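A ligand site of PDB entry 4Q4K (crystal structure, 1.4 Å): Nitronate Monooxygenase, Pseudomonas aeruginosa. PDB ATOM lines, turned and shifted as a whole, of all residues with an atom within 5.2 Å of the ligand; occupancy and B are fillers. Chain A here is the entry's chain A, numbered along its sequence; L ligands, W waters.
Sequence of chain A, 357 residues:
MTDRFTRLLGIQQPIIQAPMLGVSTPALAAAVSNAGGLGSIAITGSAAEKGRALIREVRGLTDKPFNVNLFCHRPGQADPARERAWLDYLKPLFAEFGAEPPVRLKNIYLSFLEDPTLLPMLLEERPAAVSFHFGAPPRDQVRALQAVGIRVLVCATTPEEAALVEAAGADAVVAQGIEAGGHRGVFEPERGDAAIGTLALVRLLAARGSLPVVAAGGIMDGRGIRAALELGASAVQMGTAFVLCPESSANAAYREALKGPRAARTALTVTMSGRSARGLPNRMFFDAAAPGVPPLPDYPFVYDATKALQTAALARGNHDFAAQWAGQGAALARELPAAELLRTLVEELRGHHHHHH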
ATOM      1  N   ALA A  18     -15.531  -1.944   0.466  1.00  0.00           N
ATOM      2  CA  ALA A  18     -16.380  -0.772  -0.003  1.00  0.00           C
ATOM      3  C   ALA A  18     -17.639  -1.224  -0.706  1.00  0.00           C
ATOM      4  O   ALA A  18     -17.582  -2.140  -1.502  1.00  0.00           O
ATOM      5  CB  ALA A  18     -15.593   0.142  -0.944  1.00  0.00           C
ATOM      6  N   PRO A  19     -18.790  -0.592  -0.408  1.00  0.00           N
ATOM      7  CA  PRO A  19     -19.934  -0.812  -1.278  1.00  0.00           C
ATOM      8  C   PRO A  19     -19.583  -0.249  -2.625  1.00  0.00           C
ATOM      9  O   PRO A  19     -18.981   0.797  -2.710  1.00  0.00           O
ATOM     10  CB  PRO A  19     -21.059  -0.033  -0.601  1.00  0.00           C
ATOM     11  CG  PRO A  19     -20.353   1.048   0.201  1.00  0.00           C
ATOM     12  CD  PRO A  19     -19.058   0.386   0.659  1.00  0.00           C
ATOM     13  N   MET A  20     -19.956  -0.927  -3.702  1.00  0.00           N
ATOM     14  CA  MET A  20     -19.537  -0.568  -5.059  1.00  0.00           C
ATOM     15  C   MET A  20     -20.658  -1.003  -5.949  1.00  0.00           C
ATOM     16  O   MET A  20     -20.755  -2.196  -6.328  1.00  0.00           O
ATOM     17  CB  MET A  20     -18.236  -1.270  -5.472  1.00  0.00           C
ATOM     18  CG  MET A  20     -17.046  -1.023  -4.522  1.00  0.00           C
ATOM     19  SD  MET A  20     -15.510  -1.747  -5.164  1.00  0.00           S
ATOM     20  CE  MET A  20     -15.756  -3.328  -4.341  1.00  0.00           C
ATOM     21  N   LEU A  21     -21.536  -0.071  -6.279  1.00  0.00           N
ATOM     22  CA  LEU A  21     -22.702  -0.432  -7.042  1.00  0.00           C
ATOM     23  C   LEU A  21     -22.267  -1.018  -8.394  1.00  0.00           C
ATOM     24  O   LEU A  21     -21.445  -0.442  -9.115  1.00  0.00           O
ATOM     25  CB  LEU A  21     -23.607   0.784  -7.208  1.00  0.00           C
ATOM     26  CG  LEU A  21     -24.986   0.587  -7.849  1.00  0.00           C
ATOM     27  CD1 LEU A  21     -25.894  -0.279  -6.969  1.00  0.00           C
ATOM     28  CD2 LEU A  21     -25.550   1.990  -8.055  1.00  0.00           C
ATOM     29  N   VAL A  23     -20.652  -3.805  -8.586  1.00  0.00           N
ATOM     30  CA  VAL A  23     -19.457  -4.634  -8.313  1.00  0.00           C
ATOM     31  C   VAL A  23     -19.571  -5.474  -7.052  1.00  0.00           C
ATOM     32  O   VAL A  23     -19.302  -6.669  -7.076  1.00  0.00           O
ATOM     33  CB  VAL A  23     -18.155  -3.801  -8.255  1.00  0.00           C
ATOM     34  CG1 VAL A  23     -16.971  -4.696  -7.857  1.00  0.00           C
ATOM     35  CG2 VAL A  23     -17.903  -3.110  -9.561  1.00  0.00           C
ATOM     36  N   ALA A  42     -24.416  -2.072  -2.045  1.00  0.00           N
ATOM     37  CA  ALA A  42     -25.016  -0.814  -2.435  1.00  0.00           C
ATOM     38  C   ALA A  42     -26.435  -1.106  -2.929  1.00  0.00           C
ATOM     39  O   ALA A  42     -26.632  -2.040  -3.711  1.00  0.00           O
ATOM     40  CB  ALA A  42     -24.197  -0.148  -3.563  1.00  0.00           C
ATOM     41  N   ASN A  69     -25.356   0.487   1.734  1.00  0.00           N
ATOM     42  CA  ASN A  69     -25.010   1.823   1.268  1.00  0.00           C
ATOM     43  C   ASN A  69     -26.054   2.426   0.379  1.00  0.00           C
ATOM     44  O   ASN A  69     -26.598   1.721  -0.501  1.00  0.00           O
ATOM     45  CB  ASN A  69     -23.693   1.693   0.512  1.00  0.00           C
ATOM     46  CG  ASN A  69     -23.185   2.993  -0.012  1.00  0.00           C
ATOM     47  OD1 ASN A  69     -22.613   3.840   0.738  1.00  0.00           O
ATOM     48  ND2 ASN A  69     -23.355   3.177  -1.315  1.00  0.00           N
ATOM     49  N   PHE A  71     -27.002   6.198  -1.821  1.00  0.00           N
ATOM     50  CA  PHE A  71     -26.626   7.535  -2.265  1.00  0.00           C
ATOM     51  C   PHE A  71     -27.585   8.556  -1.714  1.00  0.00           C
ATOM     52  O   PHE A  71     -28.821   8.345  -1.683  1.00  0.00           O
ATOM     53  CB  PHE A  71     -26.706   7.588  -3.806  1.00  0.00           C
ATOM     54  CG  PHE A  71     -25.754   6.674  -4.522  1.00  0.00           C
ATOM     55  CD1 PHE A  71     -24.729   5.980  -3.902  1.00  0.00           C
ATOM     56  CD2 PHE A  71     -25.867   6.571  -5.930  1.00  0.00           C
ATOM     57  CE1 PHE A  71     -23.887   5.146  -4.636  1.00  0.00           C
ATOM     58  CE2 PHE A  71     -25.042   5.740  -6.650  1.00  0.00           C
ATOM     59  CZ  PHE A  71     -24.064   5.004  -6.012  1.00  0.00           C
ATOM     60  N   HIS A 133     -23.481   8.164   0.827  1.00  0.00           N
ATOM     61  CA  HIS A 133     -22.481   8.746  -0.042  1.00  0.00           C
ATOM     62  C   HIS A 133     -23.136   9.972  -0.722  1.00  0.00           C
ATOM     63  O   HIS A 133     -24.316   9.911  -1.077  1.00  0.00           O
ATOM     64  CB  HIS A 133     -22.086   7.685  -1.104  1.00  0.00           C
ATOM     65  CG  HIS A 133     -20.762   7.951  -1.753  1.00  0.00           C
ATOM     66  ND1 HIS A 133     -19.574   7.935  -1.059  1.00  0.00           N
ATOM     67  CD2 HIS A 133     -20.435   8.195  -3.045  1.00  0.00           C
ATOM     68  CE1 HIS A 133     -18.574   8.201  -1.880  1.00  0.00           C
ATOM     69  NE2 HIS A 133     -19.072   8.394  -3.088  1.00  0.00           N
ATOM     70  N   GLN A 176     -12.751  10.019   2.424  1.00  0.00           N
ATOM     71  CA  GLN A 176     -12.432   9.545   1.097  1.00  0.00           C
ATOM     72  C   GLN A 176     -11.406  10.505   0.470  1.00  0.00           C
ATOM     73  O   GLN A 176     -11.706  11.673   0.159  1.00  0.00           O
ATOM     74  CB  GLN A 176     -13.708   9.497   0.244  1.00  0.00           C
ATOM     75  CG  GLN A 176     -13.377   8.844  -1.128  1.00  0.00           C
ATOM     76  CD  GLN A 176     -14.417   9.175  -2.169  1.00  0.00           C
ATOM     77  OE1 GLN A 176     -14.710  10.345  -2.335  1.00  0.00           O
ATOM     78  NE2 GLN A 176     -14.926   8.204  -2.897  1.00  0.00           N
ATOM     79  N   GLU A 179      -7.228   9.589  -3.907  1.00  0.00           N
ATOM     80  CA  GLU A 179      -6.830   8.261  -4.460  1.00  0.00           C
ATOM     81  C   GLU A 179      -8.012   7.395  -4.758  1.00  0.00           C
ATOM     82  O   GLU A 179      -7.851   6.441  -5.502  1.00  0.00           O
ATOM     83  CB  GLU A 179      -5.970   7.572  -3.425  1.00  0.00           C
ATOM     84  CG  GLU A 179      -4.594   8.131  -3.265  1.00  0.00           C
ATOM     85  CD  GLU A 179      -4.429   9.183  -2.205  1.00  0.00           C
ATOM     86  OE1 GLU A 179      -5.344   9.969  -1.931  1.00  0.00           O
ATOM     87  OE2 GLU A 179      -3.288   9.180  -1.732  1.00  0.00           O
ATOM     88  N   ALA A 180      -9.185   7.606  -4.153  1.00  0.00           N
ATOM     89  CA  ALA A 180     -10.244   6.603  -4.236  1.00  0.00           C
ATOM     90  C   ALA A 180     -10.785   6.377  -5.596  1.00  0.00           C
ATOM     91  O   ALA A 180     -10.864   7.302  -6.439  1.00  0.00           O
ATOM     92  CB  ALA A 180     -11.392   7.066  -3.336  1.00  0.00           C
ATOM     93  N   GLY A 181     -11.153   5.101  -5.814  1.00  0.00           N
ATOM     94  CA  GLY A 181     -11.860   4.711  -6.988  1.00  0.00           C
ATOM     95  C   GLY A 181     -13.325   5.097  -6.977  1.00  0.00           C
ATOM     96  O   GLY A 181     -13.913   5.278  -5.903  1.00  0.00           O
ATOM     97  N   GLY A 182     -13.968   5.081  -8.147  1.00  0.00           N
ATOM     98  CA  GLY A 182     -15.452   5.344  -8.172  1.00  0.00           C
ATOM     99  C   GLY A 182     -15.776   6.818  -7.866  1.00  0.00           C
ATOM    100  O   GLY A 182     -14.909   7.717  -8.055  1.00  0.00           O
ATOM    101  N   HIS A 183     -17.044   7.055  -7.602  1.00  0.00           N
ATOM    102  CA  HIS A 183     -17.491   8.445  -7.486  1.00  0.00           C
ATOM    103  C   HIS A 183     -16.921   9.175  -6.263  1.00  0.00           C
ATOM    104  O   HIS A 183     -16.949   8.594  -5.131  1.00  0.00           O
ATOM    105  CB  HIS A 183     -19.026   8.511  -7.440  1.00  0.00           C
ATOM    106  CG  HIS A 183     -19.641   8.276  -8.769  1.00  0.00           C
ATOM    107  ND1 HIS A 183     -19.654   7.044  -9.415  1.00  0.00           N
ATOM    108  CD2 HIS A 183     -20.136   9.168  -9.645  1.00  0.00           C
ATOM    109  CE1 HIS A 183     -20.233   7.199 -10.591  1.00  0.00           C
ATOM    110  NE2 HIS A 183     -20.509   8.480 -10.763  1.00  0.00           N
ATOM    111  N   ALA A 216     -10.374   5.883   3.385  1.00  0.00           N
ATOM    112  CA  ALA A 216     -10.759   5.327   2.119  1.00  0.00           C
ATOM    113  C   ALA A 216     -10.009   5.996   0.954  1.00  0.00           C
ATOM    114  O   ALA A 216     -10.089   7.219   0.780  1.00  0.00           O
ATOM    115  CB  ALA A 216     -12.261   5.530   1.898  1.00  0.00           C
ATOM    116  N   GLY A 217      -9.254   5.230   0.189  1.00  0.00           N
ATOM    117  CA  GLY A 217      -8.631   5.759  -1.022  1.00  0.00           C
ATOM    118  C   GLY A 217      -7.172   5.364  -1.103  1.00  0.00           C
ATOM    119  O   GLY A 217      -6.317   5.900  -0.403  1.00  0.00           O
ATOM    120  N   GLY A 218      -6.874   4.427  -2.034  1.00  0.00           N
ATOM    121  CA  GLY A 218      -5.514   4.029  -2.355  1.00  0.00           C
ATOM    122  C   GLY A 218      -4.922   2.908  -1.525  1.00  0.00           C
ATOM    123  O   GLY A 218      -3.747   2.570  -1.772  1.00  0.00           O
ATOM    124  N   ILE A 219      -5.679   2.382  -0.577  1.00  0.00           N
ATOM    125  CA  ILE A 219      -5.161   1.390   0.388  1.00  0.00           C
ATOM    126  C   ILE A 219      -5.358  -0.013  -0.251  1.00  0.00           C
ATOM    127  O   ILE A 219      -6.475  -0.403  -0.541  1.00  0.00           O
ATOM    128  CB  ILE A 219      -5.868   1.476   1.741  1.00  0.00           C
ATOM    129  CG1 ILE A 219      -5.537   2.864   2.383  1.00  0.00           C
ATOM    130  CG2 ILE A 219      -5.419   0.386   2.716  1.00  0.00           C
ATOM    131  CD1 ILE A 219      -6.546   3.306   3.403  1.00  0.00           C
ATOM    132  N   MET A 220      -4.246  -0.746  -0.379  1.00  0.00           N
ATOM    133  CA  MET A 220      -4.260  -2.002  -1.172  1.00  0.00           C
ATOM    134  C   MET A 220      -3.593  -3.132  -0.443  1.00  0.00           C
ATOM    135  O   MET A 220      -3.616  -4.282  -0.971  1.00  0.00           O
ATOM    136  CB  MET A 220      -3.494  -1.767  -2.465  1.00  0.00           C
ATOM    137  CG  MET A 220      -4.105  -0.723  -3.406  1.00  0.00           C
ATOM    138  SD  MET A 220      -5.789  -1.105  -3.941  1.00  0.00           S
ATOM    139  CE  MET A 220      -5.452  -2.549  -4.953  1.00  0.00           C
ATOM    140  N   GLN A 237     -11.531   1.542   4.487  1.00  0.00           N
ATOM    141  CA  GLN A 237     -12.537   1.078   3.544  1.00  0.00           C
ATOM    142  C   GLN A 237     -11.824   0.913   2.211  1.00  0.00           C
ATOM    143  O   GLN A 237     -11.080   1.809   1.755  1.00  0.00           O
ATOM    144  CB  GLN A 237     -13.690   2.078   3.440  1.00  0.00           C
ATOM    145  CG  GLN A 237     -14.771   1.683   2.438  1.00  0.00           C
ATOM    146  CD  GLN A 237     -16.073   2.430   2.622  1.00  0.00           C
ATOM    147  OE1 GLN A 237     -16.552   3.105   1.682  1.00  0.00           O
ATOM    148  NE2 GLN A 237     -16.638   2.335   3.784  1.00  0.00           N
ATOM    149  N   MET A 238     -11.917  -0.301   1.627  1.00  0.00           N
ATOM    150  CA  MET A 238     -11.157  -0.649   0.491  1.00  0.00           C
ATOM    151  C   MET A 238     -12.060  -1.219  -0.572  1.00  0.00           C
ATOM    152  O   MET A 238     -12.863  -2.134  -0.329  1.00  0.00           O
ATOM    153  CB  MET A 238     -10.146  -1.758   0.892  1.00  0.00           C
ATOM    154  CG  MET A 238      -9.077  -1.187   1.822  1.00  0.00           C
ATOM    155  SD  MET A 238      -8.087  -2.538   2.595  1.00  0.00           S
ATOM    156  CE  MET A 238      -7.267  -3.132   1.140  1.00  0.00           C
ATOM    157  N   GLY A 239     -12.009  -0.608  -1.755  1.00  0.00           N
ATOM    158  CA  GLY A 239     -12.906  -0.940  -2.847  1.00  0.00           C
ATOM    159  C   GLY A 239     -12.101  -1.621  -3.931  1.00  0.00           C
ATOM    160  O   GLY A 239     -12.324  -2.870  -4.164  1.00  0.00           O
ATOM    161  N   THR A 240     -11.185  -0.944  -4.568  1.00  0.00           N
ATOM    162  CA  THR A 240     -10.449  -1.498  -5.705  1.00  0.00           C
ATOM    163  C   THR A 240      -9.768  -2.831  -5.291  1.00  0.00           C
ATOM    164  O   THR A 240      -9.787  -3.790  -6.141  1.00  0.00           O
ATOM    165  CB  THR A 240      -9.341  -0.528  -6.116  1.00  0.00           C
ATOM    166  OG1 THR A 240      -9.930   0.732  -6.484  1.00  0.00           O
ATOM    167  CG2 THR A 240      -8.490  -1.047  -7.248  1.00  0.00           C
ATOM    168  N   ALA A 241      -9.379  -2.979  -4.035  1.00  0.00           N
ATOM    169  CA  ALA A 241      -8.680  -4.253  -3.591  1.00  0.00           C
ATOM    170  C   ALA A 241      -9.607  -5.446  -3.709  1.00  0.00           C
ATOM    171  O   ALA A 241      -9.108  -6.642  -3.858  1.00  0.00           O
ATOM    172  CB  ALA A 241      -8.162  -4.169  -2.174  1.00  0.00           C
ATOM    173  N   VAL A 243     -12.233  -5.806  -6.041  1.00  0.00           N
ATOM    174  CA  VAL A 243     -12.859  -5.923  -7.369  1.00  0.00           C
ATOM    175  C   VAL A 243     -12.509  -7.276  -8.039  1.00  0.00           C
ATOM    176  O   VAL A 243     -13.357  -7.881  -8.730  1.00  0.00           O
ATOM    177  CB  VAL A 243     -12.465  -4.728  -8.310  1.00  0.00           C
ATOM    178  CG1 VAL A 243     -12.925  -4.929  -9.757  1.00  0.00           C
ATOM    179  CG2 VAL A 243     -13.030  -3.408  -7.754  1.00  0.00           C
ATOM    180  N   TYR A 254     -13.572  -5.992 -17.368  1.00  0.00           N
ATOM    181  CA  TYR A 254     -13.153  -5.171 -16.203  1.00  0.00           C
ATOM    182  C   TYR A 254     -11.995  -5.864 -15.460  1.00  0.00           C
ATOM    183  O   TYR A 254     -10.992  -5.235 -15.133  1.00  0.00           O
ATOM    184  CB  TYR A 254     -14.376  -5.032 -15.275  1.00  0.00           C
ATOM    185  CG  TYR A 254     -14.326  -4.039 -14.112  1.00  0.00           C
ATOM    186  CD1 TYR A 254     -13.168  -3.342 -13.766  1.00  0.00           C
ATOM    187  CD2 TYR A 254     -15.493  -3.783 -13.388  1.00  0.00           C
ATOM    188  CE1 TYR A 254     -13.170  -2.457 -12.686  1.00  0.00           C
ATOM    189  CE2 TYR A 254     -15.507  -2.861 -12.331  1.00  0.00           C
ATOM    190  CZ  TYR A 254     -14.361  -2.209 -12.032  1.00  0.00           C
ATOM    191  OH  TYR A 254     -14.433  -1.328 -10.965  1.00  0.00           O
ATOM    192  N   TRP A 325     -14.197   1.308 -12.722  1.00  0.00           N
ATOM    193  CA  TRP A 325     -13.720   2.244 -11.672  1.00  0.00           C
ATOM    194  C   TRP A 325     -12.545   1.649 -10.990  1.00  0.00           C
ATOM    195  O   TRP A 325     -12.448   0.433 -10.789  1.00  0.00           O
ATOM    196  CB  TRP A 325     -14.850   2.431 -10.662  1.00  0.00           C
ATOM    197  CG  TRP A 325     -16.129   3.013 -11.297  1.00  0.00           C
ATOM    198  CD1 TRP A 325     -17.400   2.499 -11.163  1.00  0.00           C
ATOM    199  CD2 TRP A 325     -16.253   4.215 -12.054  1.00  0.00           C
ATOM    200  NE1 TRP A 325     -18.297   3.311 -11.834  1.00  0.00           N
ATOM    201  CE2 TRP A 325     -17.624   4.358 -12.400  1.00  0.00           C
ATOM    202  CE3 TRP A 325     -15.342   5.133 -12.561  1.00  0.00           C
ATOM    203  CZ2 TRP A 325     -18.106   5.438 -13.161  1.00  0.00           C
ATOM    204  CZ3 TRP A 325     -15.802   6.222 -13.354  1.00  0.00           C
ATOM    205  CH2 TRP A 325     -17.183   6.357 -13.646  1.00  0.00           C
ATOM    206  N   ALA A 326     -11.651   2.479 -10.493  1.00  0.00           N
ATOM    207  CA  ALA A 326     -10.424   1.946  -9.869  1.00  0.00           C
ATOM    208  C   ALA A 326      -9.706   3.134  -9.181  1.00  0.00           C
ATOM    209  O   ALA A 326      -9.662   4.231  -9.783  1.00  0.00           O
ATOM    210  CB  ALA A 326      -9.497   1.350 -10.968  1.00  0.00           C
ATOM    211  N   GLY A 327      -9.139   2.869  -8.007  1.00  0.00           N
ATOM    212  CA  GLY A 327      -8.330   3.815  -7.246  1.00  0.00           C
ATOM    213  C   GLY A 327      -6.912   3.984  -7.741  1.00  0.00           C
ATOM    214  O   GLY A 327      -6.400   3.232  -8.602  1.00  0.00           O
ATOM    215  N   GLN A 328      -6.197   4.938  -7.185  1.00  0.00           N
ATOM    216  CA  GLN A 328      -4.825   5.187  -7.627  1.00  0.00           C
ATOM    217  C   GLN A 328      -3.808   4.087  -7.206  1.00  0.00           C
ATOM    218  O   GLN A 328      -2.680   4.144  -7.715  1.00  0.00           O
ATOM    219  CB  GLN A 328      -4.334   6.580  -7.132  1.00  0.00           C
ATOM    220  CG  GLN A 328      -5.070   7.663  -7.900  1.00  0.00           C
ATOM    221  CD  GLN A 328      -4.666   9.104  -7.468  1.00  0.00           C
ATOM    222  OE1 GLN A 328      -4.231   9.290  -6.323  1.00  0.00           O
ATOM    223  NE2 GLN A 328      -4.785  10.068  -8.342  1.00  0.00           N
HETATM  224  N1  LIG L   1     -18.767   4.163  -2.708  1.00  0.00           N
HETATM  225  C1  LIG L   1     -20.023   4.061  -2.267  1.00  0.00           C
HETATM  226  O1  LIG L   1     -20.325   4.492  -1.016  1.00  0.00           O
HETATM  227  N2  LIG L   1     -21.022   3.609  -3.074  1.00  0.00           N
HETATM  228  C2  LIG L   1     -20.708   2.944  -4.232  1.00  0.00           C
HETATM  229  O2  LIG L   1     -21.631   2.381  -4.889  1.00  0.00           O
HETATM  230  C3  LIG L   1     -19.429   3.137  -4.783  1.00  0.00           C
HETATM  231  N3  LIG L   1     -19.075   2.601  -6.001  1.00  0.00           N
HETATM  232  C4  LIG L   1     -17.761   2.362  -6.309  1.00  0.00           C
HETATM  233  C5  LIG L   1     -17.417   1.385  -7.282  1.00  0.00           C
HETATM  234  C6  LIG L   1     -16.085   0.959  -7.427  1.00  0.00           C
HETATM  235  C7  LIG L   1     -15.696  -0.101  -8.467  1.00  0.00           C
HETATM  236  C8  LIG L   1     -15.074   1.548  -6.661  1.00  0.00           C
HETATM  237  C9  LIG L   1     -13.650   1.072  -6.766  1.00  0.00           C
HETATM  238  C10 LIG L   1     -15.447   2.466  -5.637  1.00  0.00           C
HETATM  239  C11 LIG L   1     -16.761   2.916  -5.497  1.00  0.00           C
HETATM  240  N4  LIG L   1     -17.139   3.606  -4.302  1.00  0.00           N
HETATM  241  C12 LIG L   1     -18.435   3.648  -3.924  1.00  0.00           C
HETATM  242  C13 LIG L   1     -16.081   4.275  -3.504  1.00  0.00           C
HETATM  243  C14 LIG L   1     -15.699   3.452  -2.258  1.00  0.00           C
HETATM  244  O3  LIG L   1     -16.720   3.557  -1.243  1.00  0.00           O
HETATM  245  C15 LIG L   1     -14.401   3.930  -1.620  1.00  0.00           C
HETATM  246  O4  LIG L   1     -14.489   5.375  -1.469  1.00  0.00           O
HETATM  247  C16 LIG L   1     -13.270   3.746  -2.617  1.00  0.00           C
HETATM  248  O5  LIG L   1     -13.318   2.432  -3.286  1.00  0.00           O
HETATM  249  C17 LIG L   1     -11.891   3.841  -1.878  1.00  0.00           C
HETATM  250  O6  LIG L   1     -10.783   3.821  -2.805  1.00  0.00           O
HETATM  251  P1  LIG L   1     -10.004   2.458  -3.294  1.00  0.00           P
HETATM  252  O7  LIG L   1      -8.753   2.962  -3.775  1.00  0.00           O
HETATM  253  O8  LIG L   1     -10.843   2.036  -4.408  1.00  0.00           O
HETATM  254  O9  LIG L   1     -10.039   1.497  -2.201  1.00  0.00           O
HETATM  255  O   HOH W   1      -6.598   2.059  -5.048  1.00  0.00           O
HETATM  256  O   HOH W   2     -16.086   6.363   0.362  1.00  0.00           O
HETATM  257  O   HOH W   3     -20.292   2.329  -8.502  1.00  0.00           O
HETATM  258  O   HOH W   4      -8.773  -0.830  -2.146  1.00  0.00           O
HETATM  259  O   HOH W   5      -8.890   2.429   0.162  1.00  0.00           O
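N of Thr 240 sits at hydrogen-bond distance from O8 of the ligand, at 3.0 Å.
The side-chain hydroxyl (OG1) of Thr 240 sits at hydrogen-bond distance from an oxygen (O8) of the ligand (2.6 Å).
N of Leu 21 sits at hydrogen-bond distance from O2 of the ligand.
The backbone NH of Gly 239 is in hydrogen-bond range of an oxygen (O9) of the ligand (2.9 Å).
N of Gly 218 is in hydrogen-bond range of O7 of the ligand (3.0 Å).
A nitrogen (N2) of the ligand lies close to the side-chain amide nitrogen (ND2) of Asn 69 (3.0 Å).
OE1 of Gln 237 is in hydrogen-bond range of O3 of the ligand.
O of Pro 19 lies close to N2 of the ligand (3.5 Å).
NE2 of Gln 176 is in hydrogen-bond range of O4 of the ligand, at 3.2 Å.
The backbone NH of Gly 181 is in hydrogen-bond range of an oxygen (O6) of the ligand (3.3 Å).
CB of Ala 18 touches C14 of the ligand, 3.6 Å away.
Met 20 touches the ligand.
Val 23 touches the ligand.
Ala 42 touches the ligand.
Phe 71 touches the ligand (CE1 to O2, 3.6 Å).
His 133 touches the ligand.
Glu 179 touches the ligand (O to O7, 3.99 Å).
Ala 180 touches the ligand (CA to O6, 3.2 Å).
Gly 182 touches the ligand (CA to C10, 3.8 Å).
Gly 217 touches the ligand.
CA of Met 238 touches O9 of the ligand, 3.6 Å away.
Tyr 254 touches the ligand.
Trp 325 touches the ligand.
Gly 327 touches the ligand.
Hydrophobic or aromatic side chains within 4 Å of the ligand: Ala 18, Pro 19, Met 20, Leu 21, Val 23, Ala 42, Phe 71, His 133, Ala 180 and Trp 325.
Of the 31 residues printed, 23 come within 4 Å of the ligand.
The nearest printed residue that does not touch the ligand is Ala 216 (4.03 Å).
Water W1 lies within hydrogen-bond range of O7 of the ligand (2.7 Å) and SD of Met 220 (3.4 Å).
Water W5 lies within hydrogen-bond range of O of Gln 237 (2.8 Å), O9 of the ligand (2.8 Å), N of Gly 217 (2.8 Å) and N of Ile 219 (3.3 Å).
Water W3 bridges N3 of the ligand (2.8 Å) and O of Leu 21 (3.1 Å).
The side-chain hydroxyl of Thr 240 is in hydrogen-bond range of the backbone NH of Gly 327 (2.7 Å).
OH of Tyr 254 is in hydrogen-bond range of O of Trp 325 (2.7 Å).
NE2 of Gln 176 lies within hydrogen-bond range of O of His 183, at 3.0 Å.
The backbone carbonyl oxygen (O) of His 183 lies within hydrogen-bond range of a ring nitrogen (NE2) of His 133 (3.0 Å).
N of Ala 18 is in hydrogen-bond range of O of Met 238 (2.8 Å).
The backbone NH (N) of Gln 328 is in hydrogen-bond range of the backbone carbonyl oxygen (O) of Glu 179 (2.8 Å).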
